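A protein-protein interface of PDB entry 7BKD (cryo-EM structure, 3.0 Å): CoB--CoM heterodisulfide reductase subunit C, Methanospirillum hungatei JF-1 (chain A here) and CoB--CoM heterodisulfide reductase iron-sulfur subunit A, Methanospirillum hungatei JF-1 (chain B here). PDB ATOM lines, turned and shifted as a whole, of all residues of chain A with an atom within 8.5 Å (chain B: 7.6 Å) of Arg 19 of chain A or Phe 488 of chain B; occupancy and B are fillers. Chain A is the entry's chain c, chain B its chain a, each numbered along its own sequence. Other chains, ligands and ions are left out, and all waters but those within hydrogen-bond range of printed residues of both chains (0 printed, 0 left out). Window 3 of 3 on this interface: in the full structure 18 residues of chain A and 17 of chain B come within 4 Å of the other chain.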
ATOM      1  N   ALA A   2      25.800 -30.871  15.352  1.00  0.00           N
ATOM      2  CA  ALA A   2      25.484 -29.458  15.202  1.00  0.00           C
ATOM      3  C   ALA A   2      24.049 -29.256  14.734  1.00  0.00           C
ATOM      4  O   ALA A   2      23.680 -28.164  14.305  1.00  0.00           O
ATOM      5  CB  ALA A   2      26.454 -28.801  14.233  1.00  0.00           C
ATOM      6  N   ALA A  16      29.457 -29.613  18.660  1.00  0.00           N
ATOM      7  CA  ALA A  16      29.347 -28.161  18.713  1.00  0.00           C
ATOM      8  C   ALA A  16      29.257 -27.586  17.306  1.00  0.00           C
ATOM      9  O   ALA A  16      29.941 -28.042  16.387  1.00  0.00           O
ATOM     10  CB  ALA A  16      30.546 -27.566  19.447  1.00  0.00           C
ATOM     11  N   ASP A  17      28.398 -26.587  17.134  1.00  0.00           N
ATOM     12  CA  ASP A  17      28.254 -25.953  15.832  1.00  0.00           C
ATOM     13  C   ASP A  17      29.505 -25.141  15.523  1.00  0.00           C
ATOM     14  O   ASP A  17      29.820 -24.179  16.228  1.00  0.00           O
ATOM     15  CB  ASP A  17      27.014 -25.066  15.802  1.00  0.00           C
ATOM     16  CG  ASP A  17      26.526 -24.794  14.389  1.00  0.00           C
ATOM     17  OD1 ASP A  17      27.344 -24.848  13.446  1.00  0.00           O
ATOM     18  OD2 ASP A  17      25.320 -24.521  14.221  1.00  0.00           O
ATOM     19  N   ARG A  18      30.218 -25.531  14.470  1.00  0.00           N
ATOM     20  CA  ARG A  18      31.452 -24.869  14.079  1.00  0.00           C
ATOM     21  C   ARG A  18      31.241 -23.734  13.085  1.00  0.00           C
ATOM     22  O   ARG A  18      32.212 -23.060  12.728  1.00  0.00           O
ATOM     23  CB  ARG A  18      32.426 -25.888  13.477  1.00  0.00           C
ATOM     24  CG  ARG A  18      33.437 -26.452  14.455  1.00  0.00           C
ATOM     25  CD  ARG A  18      32.831 -27.542  15.313  1.00  0.00           C
ATOM     26  NE  ARG A  18      33.837 -28.476  15.804  1.00  0.00           N
ATOM     27  CZ  ARG A  18      33.558 -29.572  16.500  1.00  0.00           C
ATOM     28  NH1 ARG A  18      34.535 -30.371  16.902  1.00  0.00           N
ATOM     29  NH2 ARG A  18      32.301 -29.871  16.791  1.00  0.00           N
ATOM     30  N   ARG A  19      30.011 -23.501  12.633  1.00  0.00           N
ATOM     31  CA  ARG A  19      29.757 -22.492  11.616  1.00  0.00           C
ATOM     32  C   ARG A  19      29.642 -21.108  12.237  1.00  0.00           C
ATOM     33  O   ARG A  19      28.867 -20.899  13.174  1.00  0.00           O
ATOM     34  CB  ARG A  19      28.479 -22.805  10.842  1.00  0.00           C
ATOM     35  CG  ARG A  19      28.696 -23.479   9.510  1.00  0.00           C
ATOM     36  CD  ARG A  19      27.364 -23.778   8.856  1.00  0.00           C
ATOM     37  NE  ARG A  19      27.502 -24.611   7.669  1.00  0.00           N
ATOM     38  CZ  ARG A  19      26.580 -25.476   7.264  1.00  0.00           C
ATOM     39  NH1 ARG A  19      25.458 -25.616   7.955  1.00  0.00           N
ATOM     40  NH2 ARG A  19      26.780 -26.201   6.175  1.00  0.00           N
ATOM     41  N   TYR A  20      30.400 -20.160  11.696  1.00  0.00           N
ATOM     42  CA  TYR A  20      30.231 -18.766  12.077  1.00  0.00           C
ATOM     43  C   TYR A  20      28.902 -18.255  11.537  1.00  0.00           C
ATOM     44  O   TYR A  20      28.601 -18.417  10.351  1.00  0.00           O
ATOM     45  CB  TYR A  20      31.386 -17.921  11.547  1.00  0.00           C
ATOM     46  CG  TYR A  20      31.140 -16.432  11.650  1.00  0.00           C
ATOM     47  CD1 TYR A  20      31.360 -15.755  12.841  1.00  0.00           C
ATOM     48  CD2 TYR A  20      30.680 -15.705  10.560  1.00  0.00           C
ATOM     49  CE1 TYR A  20      31.131 -14.400  12.942  1.00  0.00           C
ATOM     50  CE2 TYR A  20      30.447 -14.349  10.652  1.00  0.00           C
ATOM     51  CZ  TYR A  20      30.676 -13.701  11.846  1.00  0.00           C
ATOM     52  OH  TYR A  20      30.450 -12.349  11.945  1.00  0.00           O
ATOM     53  N   HIS A  21      28.111 -17.647  12.408  1.00  0.00           N
ATOM     54  CA  HIS A  21      26.860 -17.004  12.049  1.00  0.00           C
ATOM     55  C   HIS A  21      26.960 -15.516  12.345  1.00  0.00           C
ATOM     56  O   HIS A  21      27.780 -15.078  13.154  1.00  0.00           O
ATOM     57  CB  HIS A  21      25.685 -17.617  12.814  1.00  0.00           C
ATOM     58  CG  HIS A  21      25.249 -18.946  12.286  1.00  0.00           C
ATOM     59  ND1 HIS A  21      25.228 -19.244  10.942  1.00  0.00           N
ATOM     60  CD2 HIS A  21      24.828 -20.064  12.925  1.00  0.00           C
ATOM     61  CE1 HIS A  21      24.805 -20.482  10.773  1.00  0.00           C
ATOM     62  NE2 HIS A  21      24.555 -21.003  11.961  1.00  0.00           N
ATOM     63  N   LEU A  22      26.121 -14.732  11.669  1.00  0.00           N
ATOM     64  CA  LEU A  22      26.128 -13.293  11.903  1.00  0.00           C
ATOM     65  C   LEU A  22      25.553 -12.919  13.259  1.00  0.00           C
ATOM     66  O   LEU A  22      25.747 -11.784  13.705  1.00  0.00           O
ATOM     67  CB  LEU A  22      25.364 -12.581  10.789  1.00  0.00           C
ATOM     68  CG  LEU A  22      26.131 -12.561   9.470  1.00  0.00           C
ATOM     69  CD1 LEU A  22      25.482 -11.620   8.488  1.00  0.00           C
ATOM     70  CD2 LEU A  22      27.585 -12.188   9.697  1.00  0.00           C
ATOM     71  N   SER A  23      24.854 -13.838  13.921  1.00  0.00           N
ATOM     72  CA  SER A  23      24.460 -13.639  15.307  1.00  0.00           C
ATOM     73  C   SER A  23      25.611 -13.867  16.274  1.00  0.00           C
ATOM     74  O   SER A  23      25.475 -13.555  17.462  1.00  0.00           O
ATOM     75  CB  SER A  23      23.302 -14.572  15.660  1.00  0.00           C
ATOM     76  OG  SER A  23      22.327 -14.579  14.634  1.00  0.00           O
ATOM     77  N   ASP A  24      26.734 -14.403  15.796  1.00  0.00           N
ATOM     78  CA  ASP A  24      27.908 -14.623  16.628  1.00  0.00           C
ATOM     79  C   ASP A  24      28.734 -13.362  16.812  1.00  0.00           C
ATOM     80  O   ASP A  24      29.692 -13.373  17.592  1.00  0.00           O
ATOM     81  CB  ASP A  24      28.787 -15.716  16.014  1.00  0.00           C
ATOM     82  CG  ASP A  24      28.144 -17.085  16.072  1.00  0.00           C
ATOM     83  OD1 ASP A  24      27.349 -17.332  17.003  1.00  0.00           O
ATOM     84  OD2 ASP A  24      28.434 -17.912  15.183  1.00  0.00           O
ATOM     85  N   LEU A  75      34.131 -11.785  17.876  1.00  0.00           N
ATOM     86  CA  LEU A  75      33.819 -13.096  18.437  1.00  0.00           C
ATOM     87  C   LEU A  75      34.268 -13.163  19.895  1.00  0.00           C
ATOM     88  O   LEU A  75      35.255 -13.804  20.253  1.00  0.00           O
ATOM     89  CB  LEU A  75      34.463 -14.194  17.600  1.00  0.00           C
ATOM     90  CG  LEU A  75      33.854 -14.379  16.210  1.00  0.00           C
ATOM     91  CD1 LEU A  75      34.639 -15.396  15.414  1.00  0.00           C
ATOM     92  CD2 LEU A  75      32.406 -14.793  16.335  1.00  0.00           C
ATOM     93  N   GLU A  78      34.823 -16.435  22.506  1.00  0.00           N
ATOM     94  CA  GLU A  78      35.796 -17.266  21.812  1.00  0.00           C
ATOM     95  C   GLU A  78      37.222 -16.783  22.010  1.00  0.00           C
ATOM     96  O   GLU A  78      38.116 -17.595  22.255  1.00  0.00           O
ATOM     97  CB  GLU A  78      35.475 -17.318  20.315  1.00  0.00           C
ATOM     98  CG  GLU A  78      36.442 -18.148  19.493  1.00  0.00           C
ATOM     99  CD  GLU A  78      35.909 -18.461  18.111  1.00  0.00           C
ATOM    100  OE1 GLU A  78      34.692 -18.279  17.891  1.00  0.00           O
ATOM    101  OE2 GLU A  78      36.704 -18.890  17.246  1.00  0.00           O
ATOM    102  N   GLU B 356      24.343 -23.587  -8.134  1.00  0.00           N
ATOM    103  CA  GLU B 356      24.560 -23.443  -6.699  1.00  0.00           C
ATOM    104  C   GLU B 356      24.312 -22.023  -6.213  1.00  0.00           C
ATOM    105  O   GLU B 356      24.143 -21.817  -5.009  1.00  0.00           O
ATOM    106  CB  GLU B 356      25.976 -23.881  -6.332  1.00  0.00           C
ATOM    107  CG  GLU B 356      27.060 -22.951  -6.845  1.00  0.00           C
ATOM    108  CD  GLU B 356      27.469 -23.251  -8.270  1.00  0.00           C
ATOM    109  OE1 GLU B 356      26.729 -23.974  -8.971  1.00  0.00           O
ATOM    110  OE2 GLU B 356      28.531 -22.754  -8.691  1.00  0.00           O
ATOM    111  N   TRP B 357      24.290 -21.045  -7.115  1.00  0.00           N
ATOM    112  CA  TRP B 357      23.863 -19.690  -6.794  1.00  0.00           C
ATOM    113  C   TRP B 357      22.571 -19.459  -7.565  1.00  0.00           C
ATOM    114  O   TRP B 357      22.593 -19.317  -8.793  1.00  0.00           O
ATOM    115  CB  TRP B 357      24.930 -18.667  -7.170  1.00  0.00           C
ATOM    116  CG  TRP B 357      26.283 -19.035  -6.669  1.00  0.00           C
ATOM    117  CD1 TRP B 357      26.634 -19.306  -5.383  1.00  0.00           C
ATOM    118  CD2 TRP B 357      27.485 -19.123  -7.441  1.00  0.00           C
ATOM    119  NE1 TRP B 357      27.972 -19.598  -5.309  1.00  0.00           N
ATOM    120  CE2 TRP B 357      28.520 -19.486  -6.558  1.00  0.00           C
ATOM    121  CE3 TRP B 357      27.785 -18.942  -8.794  1.00  0.00           C
ATOM    122  CZ2 TRP B 357      29.830 -19.670  -6.982  1.00  0.00           C
ATOM    123  CZ3 TRP B 357      29.087 -19.129  -9.214  1.00  0.00           C
ATOM    124  CH2 TRP B 357      30.094 -19.488  -8.311  1.00  0.00           C
ATOM    125  N   PHE B 443      32.473 -11.979  -0.136  1.00  0.00           N
ATOM    126  CA  PHE B 443      33.046 -13.320  -0.151  1.00  0.00           C
ATOM    127  C   PHE B 443      34.040 -13.358  -1.298  1.00  0.00           C
ATOM    128  O   PHE B 443      33.665 -13.530  -2.459  1.00  0.00           O
ATOM    129  CB  PHE B 443      31.953 -14.367  -0.288  1.00  0.00           C
ATOM    130  CG  PHE B 443      30.900 -14.264   0.764  1.00  0.00           C
ATOM    131  CD1 PHE B 443      31.101 -14.818   2.011  1.00  0.00           C
ATOM    132  CD2 PHE B 443      29.716 -13.594   0.516  1.00  0.00           C
ATOM    133  CE1 PHE B 443      30.137 -14.718   2.987  1.00  0.00           C
ATOM    134  CE2 PHE B 443      28.751 -13.494   1.488  1.00  0.00           C
ATOM    135  CZ  PHE B 443      28.963 -14.057   2.726  1.00  0.00           C
ATOM    136  N   GLY B 471      36.762 -16.564   1.197  1.00  0.00           N
ATOM    137  CA  GLY B 471      36.271 -17.870   0.819  1.00  0.00           C
ATOM    138  C   GLY B 471      35.309 -17.815  -0.348  1.00  0.00           C
ATOM    139  O   GLY B 471      34.366 -17.020  -0.349  1.00  0.00           O
ATOM    140  N   ARG B 472      35.546 -18.654  -1.351  1.00  0.00           N
ATOM    141  CA  ARG B 472      34.629 -18.754  -2.475  1.00  0.00           C
ATOM    142  C   ARG B 472      33.317 -19.377  -2.024  1.00  0.00           C
ATOM    143  O   ARG B 472      33.303 -20.386  -1.315  1.00  0.00           O
ATOM    144  CB  ARG B 472      35.256 -19.581  -3.594  1.00  0.00           C
ATOM    145  CG  ARG B 472      34.526 -19.492  -4.916  1.00  0.00           C
ATOM    146  CD  ARG B 472      35.286 -20.225  -6.002  1.00  0.00           C
ATOM    147  NE  ARG B 472      34.487 -20.393  -7.208  1.00  0.00           N
ATOM    148  CZ  ARG B 472      33.565 -21.334  -7.367  1.00  0.00           C
ATOM    149  NH1 ARG B 472      33.323 -22.197  -6.395  1.00  0.00           N
ATOM    150  NH2 ARG B 472      32.885 -21.413  -8.501  1.00  0.00           N
ATOM    151  N   VAL B 473      32.208 -18.767  -2.437  1.00  0.00           N
ATOM    152  CA  VAL B 473      30.896 -19.217  -1.996  1.00  0.00           C
ATOM    153  C   VAL B 473      30.650 -20.634  -2.490  1.00  0.00           C
ATOM    154  O   VAL B 473      30.777 -20.925  -3.686  1.00  0.00           O
ATOM    155  CB  VAL B 473      29.801 -18.259  -2.489  1.00  0.00           C
ATOM    156  CG1 VAL B 473      28.429 -18.836  -2.201  1.00  0.00           C
ATOM    157  CG2 VAL B 473      29.954 -16.911  -1.826  1.00  0.00           C
ATOM    158  N   ALA B 474      30.302 -21.526  -1.565  1.00  0.00           N
ATOM    159  CA  ALA B 474      30.001 -22.902  -1.940  1.00  0.00           C
ATOM    160  C   ALA B 474      28.600 -23.006  -2.523  1.00  0.00           C
ATOM    161  O   ALA B 474      28.424 -23.462  -3.657  1.00  0.00           O
ATOM    162  CB  ALA B 474      30.161 -23.836  -0.740  1.00  0.00           C
ATOM    163  N   ASN B 475      27.588 -22.576  -1.772  1.00  0.00           N
ATOM    164  CA  ASN B 475      26.244 -22.618  -2.336  1.00  0.00           C
ATOM    165  C   ASN B 475      25.344 -21.643  -1.595  1.00  0.00           C
ATOM    166  O   ASN B 475      25.737 -21.022  -0.605  1.00  0.00           O
ATOM    167  CB  ASN B 475      25.664 -24.042  -2.318  1.00  0.00           C
ATOM    168  CG  ASN B 475      25.134 -24.447  -0.965  1.00  0.00           C
ATOM    169  OD1 ASN B 475      25.888 -24.579  -0.004  1.00  0.00           O
ATOM    170  ND2 ASN B 475      23.830 -24.649  -0.880  1.00  0.00           N
ATOM    171  N   VAL B 476      24.133 -21.485  -2.122  1.00  0.00           N
ATOM    172  CA  VAL B 476      23.171 -20.510  -1.630  1.00  0.00           C
ATOM    173  C   VAL B 476      21.818 -21.190  -1.487  1.00  0.00           C
ATOM    174  O   VAL B 476      21.336 -21.826  -2.430  1.00  0.00           O
ATOM    175  CB  VAL B 476      23.064 -19.292  -2.570  1.00  0.00           C
ATOM    176  CG1 VAL B 476      22.057 -18.302  -2.039  1.00  0.00           C
ATOM    177  CG2 VAL B 476      24.416 -18.631  -2.758  1.00  0.00           C
ATOM    178  N   LEU B 477      21.209 -21.049  -0.317  1.00  0.00           N
ATOM    179  CA  LEU B 477      19.844 -21.488  -0.074  1.00  0.00           C
ATOM    180  C   LEU B 477      18.990 -20.272   0.260  1.00  0.00           C
ATOM    181  O   LEU B 477      19.501 -19.173   0.456  1.00  0.00           O
ATOM    182  CB  LEU B 477      19.784 -22.519   1.060  1.00  0.00           C
ATOM    183  CG  LEU B 477      20.652 -23.767   0.908  1.00  0.00           C
ATOM    184  CD1 LEU B 477      20.501 -24.669   2.120  1.00  0.00           C
ATOM    185  CD2 LEU B 477      20.313 -24.515  -0.371  1.00  0.00           C
ATOM    186  N   GLU B 478      17.677 -20.461   0.321  1.00  0.00           N
ATOM    187  CA  GLU B 478      16.802 -19.378   0.743  1.00  0.00           C
ATOM    188  C   GLU B 478      15.737 -19.907   1.691  1.00  0.00           C
ATOM    189  O   GLU B 478      15.301 -21.056   1.584  1.00  0.00           O
ATOM    190  CB  GLU B 478      16.126 -18.670  -0.443  1.00  0.00           C
ATOM    191  CG  GLU B 478      14.891 -19.362  -0.967  1.00  0.00           C
ATOM    192  CD  GLU B 478      14.363 -18.736  -2.240  1.00  0.00           C
ATOM    193  OE1 GLU B 478      13.799 -19.472  -3.078  1.00  0.00           O
ATOM    194  OE2 GLU B 478      14.506 -17.506  -2.401  1.00  0.00           O
ATOM    195  N   LEU B 485      18.724 -14.996   2.076  1.00  0.00           N
ATOM    196  CA  LEU B 485      19.612 -15.892   1.357  1.00  0.00           C
ATOM    197  C   LEU B 485      20.688 -16.363   2.323  1.00  0.00           C
ATOM    198  O   LEU B 485      21.406 -15.544   2.906  1.00  0.00           O
ATOM    199  CB  LEU B 485      20.235 -15.198   0.143  1.00  0.00           C
ATOM    200  CG  LEU B 485      19.401 -15.124  -1.146  1.00  0.00           C
ATOM    201  CD1 LEU B 485      19.095 -16.490  -1.731  1.00  0.00           C
ATOM    202  CD2 LEU B 485      18.131 -14.308  -0.971  1.00  0.00           C
ATOM    203  N   HIS B 486      20.780 -17.675   2.502  1.00  0.00           N
ATOM    204  CA  HIS B 486      21.845 -18.294   3.277  1.00  0.00           C
ATOM    205  C   HIS B 486      23.009 -18.592   2.348  1.00  0.00           C
ATOM    206  O   HIS B 486      22.872 -19.386   1.412  1.00  0.00           O
ATOM    207  CB  HIS B 486      21.362 -19.582   3.936  1.00  0.00           C
ATOM    208  CG  HIS B 486      20.415 -19.363   5.069  1.00  0.00           C
ATOM    209  ND1 HIS B 486      19.201 -18.728   4.911  1.00  0.00           N
ATOM    210  CD2 HIS B 486      20.498 -19.699   6.376  1.00  0.00           C
ATOM    211  CE1 HIS B 486      18.581 -18.682   6.075  1.00  0.00           C
ATOM    212  NE2 HIS B 486      19.346 -19.262   6.981  1.00  0.00           N
ATOM    213  N   VAL B 487      24.146 -17.958   2.604  1.00  0.00           N
ATOM    214  CA  VAL B 487      25.359 -18.165   1.829  1.00  0.00           C
ATOM    215  C   VAL B 487      26.257 -19.095   2.628  1.00  0.00           C
ATOM    216  O   VAL B 487      26.656 -18.768   3.752  1.00  0.00           O
ATOM    217  CB  VAL B 487      26.061 -16.832   1.528  1.00  0.00           C
ATOM    218  CG1 VAL B 487      27.376 -17.066   0.810  1.00  0.00           C
ATOM    219  CG2 VAL B 487      25.148 -15.934   0.717  1.00  0.00           C
ATOM    220  N   PHE B 488      26.565 -20.258   2.063  1.00  0.00           N
ATOM    221  CA  PHE B 488      27.399 -21.256   2.710  1.00  0.00           C
ATOM    222  C   PHE B 488      28.750 -21.282   2.020  1.00  0.00           C
ATOM    223  O   PHE B 488      28.825 -21.493   0.799  1.00  0.00           O
ATOM    224  CB  PHE B 488      26.746 -22.636   2.659  1.00  0.00           C
ATOM    225  CG  PHE B 488      25.483 -22.729   3.449  1.00  0.00           C
ATOM    226  CD1 PHE B 488      25.509 -23.115   4.774  1.00  0.00           C
ATOM    227  CD2 PHE B 488      24.267 -22.422   2.869  1.00  0.00           C
ATOM    228  CE1 PHE B 488      24.347 -23.199   5.504  1.00  0.00           C
ATOM    229  CE2 PHE B 488      23.102 -22.505   3.596  1.00  0.00           C
ATOM    230  CZ  PHE B 488      23.141 -22.890   4.914  1.00  0.00           C
ATOM    231  N   THR B 489      29.803 -21.067   2.803  1.00  0.00           N
ATOM    232  CA  THR B 489      31.173 -21.152   2.315  1.00  0.00           C
ATOM    233  C   THR B 489      32.075 -21.475   3.499  1.00  0.00           C
ATOM    234  O   THR B 489      31.602 -21.841   4.576  1.00  0.00           O
ATOM    235  CB  THR B 489      31.596 -19.858   1.607  1.00  0.00           C
ATOM    236  OG1 THR B 489      32.966 -19.958   1.202  1.00  0.00           O
ATOM    237  CG2 THR B 489      31.429 -18.658   2.522  1.00  0.00           C
ATOM    238  N   GLU B 490      33.380 -21.371   3.292  1.00  0.00           N
ATOM    239  CA  GLU B 490      34.344 -21.372   4.377  1.00  0.00           C
ATOM    240  C   GLU B 490      34.963 -19.987   4.467  1.00  0.00           C
ATOM    241  O   GLU B 490      35.169 -19.323   3.449  1.00  0.00           O
ATOM    242  CB  GLU B 490      35.474 -22.381   4.159  1.00  0.00           C
ATOM    243  CG  GLU B 490      36.430 -22.458   5.346  1.00  0.00           C
ATOM    244  CD  GLU B 490      37.581 -23.416   5.138  1.00  0.00           C
ATOM    245  OE1 GLU B 490      37.688 -23.988   4.039  1.00  0.00           O
ATOM    246  OE2 GLU B 490      38.373 -23.609   6.084  1.00  0.00           O
ATOM    247  N   ARG B 496      37.064 -21.743   9.265  1.00  0.00           N
ATOM    248  CA  ARG B 496      35.815 -22.299   9.769  1.00  0.00           C
ATOM    249  C   ARG B 496      34.728 -22.215   8.710  1.00  0.00           C
ATOM    250  O   ARG B 496      34.696 -21.264   7.923  1.00  0.00           O
ATOM    251  CB  ARG B 496      35.338 -21.575  11.039  1.00  0.00           C
ATOM    252  CG  ARG B 496      35.862 -22.167  12.334  1.00  0.00           C
ATOM    253  CD  ARG B 496      35.679 -21.202  13.496  1.00  0.00           C
ATOM    254  NE  ARG B 496      34.271 -21.031  13.828  1.00  0.00           N
ATOM    255  CZ  ARG B 496      33.800 -20.083  14.629  1.00  0.00           C
ATOM    256  NH1 ARG B 496      34.626 -19.210  15.186  1.00  0.00           N
ATOM    257  NH2 ARG B 496      32.501 -20.006  14.870  1.00  0.00           N
ATOM    258  N   PRO B 497      33.816 -23.185   8.680  1.00  0.00           N
ATOM    259  CA  PRO B 497      32.631 -23.045   7.830  1.00  0.00           C
ATOM    260  C   PRO B 497      31.791 -21.858   8.272  1.00  0.00           C
ATOM    261  O   PRO B 497      31.781 -21.478   9.443  1.00  0.00           O
ATOM    262  CB  PRO B 497      31.886 -24.371   8.030  1.00  0.00           C
ATOM    263  CG  PRO B 497      32.447 -24.945   9.285  1.00  0.00           C
ATOM    264  CD  PRO B 497      33.868 -24.499   9.338  1.00  0.00           C
ATOM    265  N   VAL B 498      31.094 -21.256   7.311  1.00  0.00           N
ATOM    266  CA  VAL B 498      30.374 -20.005   7.508  1.00  0.00           C
ATOM    267  C   VAL B 498      29.030 -20.097   6.800  1.00  0.00           C
ATOM    268  O   VAL B 498      28.957 -20.530   5.643  1.00  0.00           O
ATOM    269  CB  VAL B 498      31.175 -18.797   6.977  1.00  0.00           C
ATOM    270  CG1 VAL B 498      30.410 -17.520   7.188  1.00  0.00           C
ATOM    271  CG2 VAL B 498      32.523 -18.705   7.651  1.00  0.00           C
ATOM    272  N   ASP B 499      27.972 -19.672   7.495  1.00  0.00           N
ATOM    273  CA  ASP B 499      26.627 -19.542   6.938  1.00  0.00           C
ATOM    274  C   ASP B 499      26.141 -18.126   7.234  1.00  0.00           C
ATOM    275  O   ASP B 499      25.800 -17.806   8.377  1.00  0.00           O
ATOM    276  CB  ASP B 499      25.674 -20.580   7.521  1.00  0.00           C
ATOM    277  CG  ASP B 499      24.223 -20.289   7.183  1.00  0.00           C
ATOM    278  OD1 ASP B 499      23.354 -20.471   8.061  1.00  0.00           O
ATOM    279  OD2 ASP B 499      23.949 -19.881   6.035  1.00  0.00           O
ATOM    280  N   VAL B 500      26.087 -17.288   6.207  1.00  0.00           N
ATOM    281  CA  VAL B 500      25.777 -15.872   6.370  1.00  0.00           C
ATOM    282  C   VAL B 500      24.385 -15.602   5.814  1.00  0.00           C
ATOM    283  O   VAL B 500      24.100 -15.909   4.652  1.00  0.00           O
ATOM    284  CB  VAL B 500      26.830 -14.987   5.682  1.00  0.00           C
ATOM    285  CG1 VAL B 500      26.309 -13.575   5.493  1.00  0.00           C
ATOM    286  CG2 VAL B 500      28.105 -14.960   6.493  1.00  0.00           C
ATOM    287  N   GLU B 501      23.514 -15.048   6.652  1.00  0.00           N
ATOM    288  CA  GLU B 501      22.255 -14.482   6.192  1.00  0.00           C
ATOM    289  C   GLU B 501      22.526 -13.202   5.417  1.00  0.00           C
ATOM    290  O   GLU B 501      23.370 -12.397   5.814  1.00  0.00           O
ATOM    291  CB  GLU B 501      21.345 -14.149   7.373  1.00  0.00           C
ATOM    292  CG  GLU B 501      21.077 -15.266   8.347  1.00  0.00           C
ATOM    293  CD  GLU B 501      20.147 -16.301   7.786  1.00  0.00           C
ATOM    294  OE1 GLU B 501      19.350 -15.946   6.894  1.00  0.00           O
ATOM    295  OE2 GLU B 501      20.199 -17.457   8.254  1.00  0.00           O
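Hydrophobic or aromatic side chains of chain B within 4 Å of the printed part of chain A: Phe 488, Pro 497, Val 498 and Val 500.
Of the 12 printed residues of chain A, 7 touch a printed residue of chain B.
Hydrophobic or aromatic side chains of chain A within 4 Å of the printed part of chain B: Tyr 20, His 21, Leu 22 and Leu 75.
Among the printed residues, 15 pairs touch across the chains.
Among the printed residues, Asp or Glu carboxylates within 4 Å of a Lys or Arg side-chain nitrogen of the other chain: Glu 78 of chain A with Arg 496 of chain B.
O of Arg 18 of chain A touches O of Pro 497 of chain B, at 3.7 Å.
Phe 488 of chain B touches Arg 19 of chain A.
CA of Arg 19 of chain A touches O of Pro 497 of chain B, at 3.1 Å.
Arg 19 of chain A touches Val 498 of chain B.
CB of Asp 499 of chain B touches CD of Arg 19 of chain A (3.9 Å).
Tyr 20 of chain A touches Arg 496 of chain B.
Tyr 20 of chain A touches Val 498 of chain B (O to CA, 3.7 Å).
CD1 of Leu 22 of chain A touches CG1 of Val 500 of chain B (3.7 Å).
Glu 501 of chain B touches Leu 22 of chain A (O to CD1, 3.5 Å).
CD1 of Leu 75 of chain A touches NH1 of Arg 496 of chain B, 3.8 Å away.
O of Arg 18 of chain A is in hydrogen-bond range of NE of Arg 496 of chain B, 3.1 Å away.
The side-chain carboxylate (OE1) of Glu 78 of chain A is in salt-bridge range of the guanidinium group (NH1) of Arg 496 of chain B (2.9 Å).
N of Tyr 20 of chain A lies within hydrogen-bond range of O of Pro 497 of chain B, at 3.0 Å.
N of Asp 499 of chain B lies within hydrogen-bond range of O of Tyr 20 of chain A.
O of Asp 499 of chain B is in hydrogen-bond range of ND1 of His 21 of chain A (3.0 Å).
The backbone carbonyl oxygen (O) of Phe 488 of chain B is in hydrogen-bond range of the backbone NH (N) of Ala 474 of chain B, 2.8 Å away.
N of Phe 488 of chain B sits at hydrogen-bond distance from O of Asn 475 of chain B (2.9 Å).
N of Val 487 of chain B sits at hydrogen-bond distance from O of Val 500 of chain B (2.9 Å).
The backbone carbonyl oxygen (O) of Thr 489 of chain B lies within hydrogen-bond range of the backbone NH (N) of Val 498 of chain B, at 2.8 Å.
The backbone carbonyl oxygen (O) of Ala 16 of chain A lies within hydrogen-bond range of the guanidinium group (NH2) of Arg 18 of chain A (3.0 Å).
OD2 of Asp 24 of chain A is in hydrogen-bond range of N of His 21 of chain A (2.8 Å).
Of chain B, only Phe 488, Pro 497, Val 498 and Asp 499 come within 4 Å of Arg 19 of chain A.
Printed residues of chain B within 4 Å of Leu 22 of chain A: Val 500 and Glu 501.
Printed residues of chain A within 4 Å of Phe 488 of chain B: Arg 19.
Thr 489 of chain B touches none of the printed residues of chain A.
Printed residues of chain A within 4 Å of Arg 496 of chain B: Arg 18, Tyr 20, Leu 75 and Glu 78.
Printed residues of chain A within 4 Å of Glu 501 of chain B: Leu 22 (3.5 Å).
The nearest residue of chain B that does not touch Arg 19 of chain A is Arg 496 of chain B (4.04 Å).
The nearest residue of chain A that does not touch Phe 488 of chain B is His 21 of chain A (5.9 Å).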
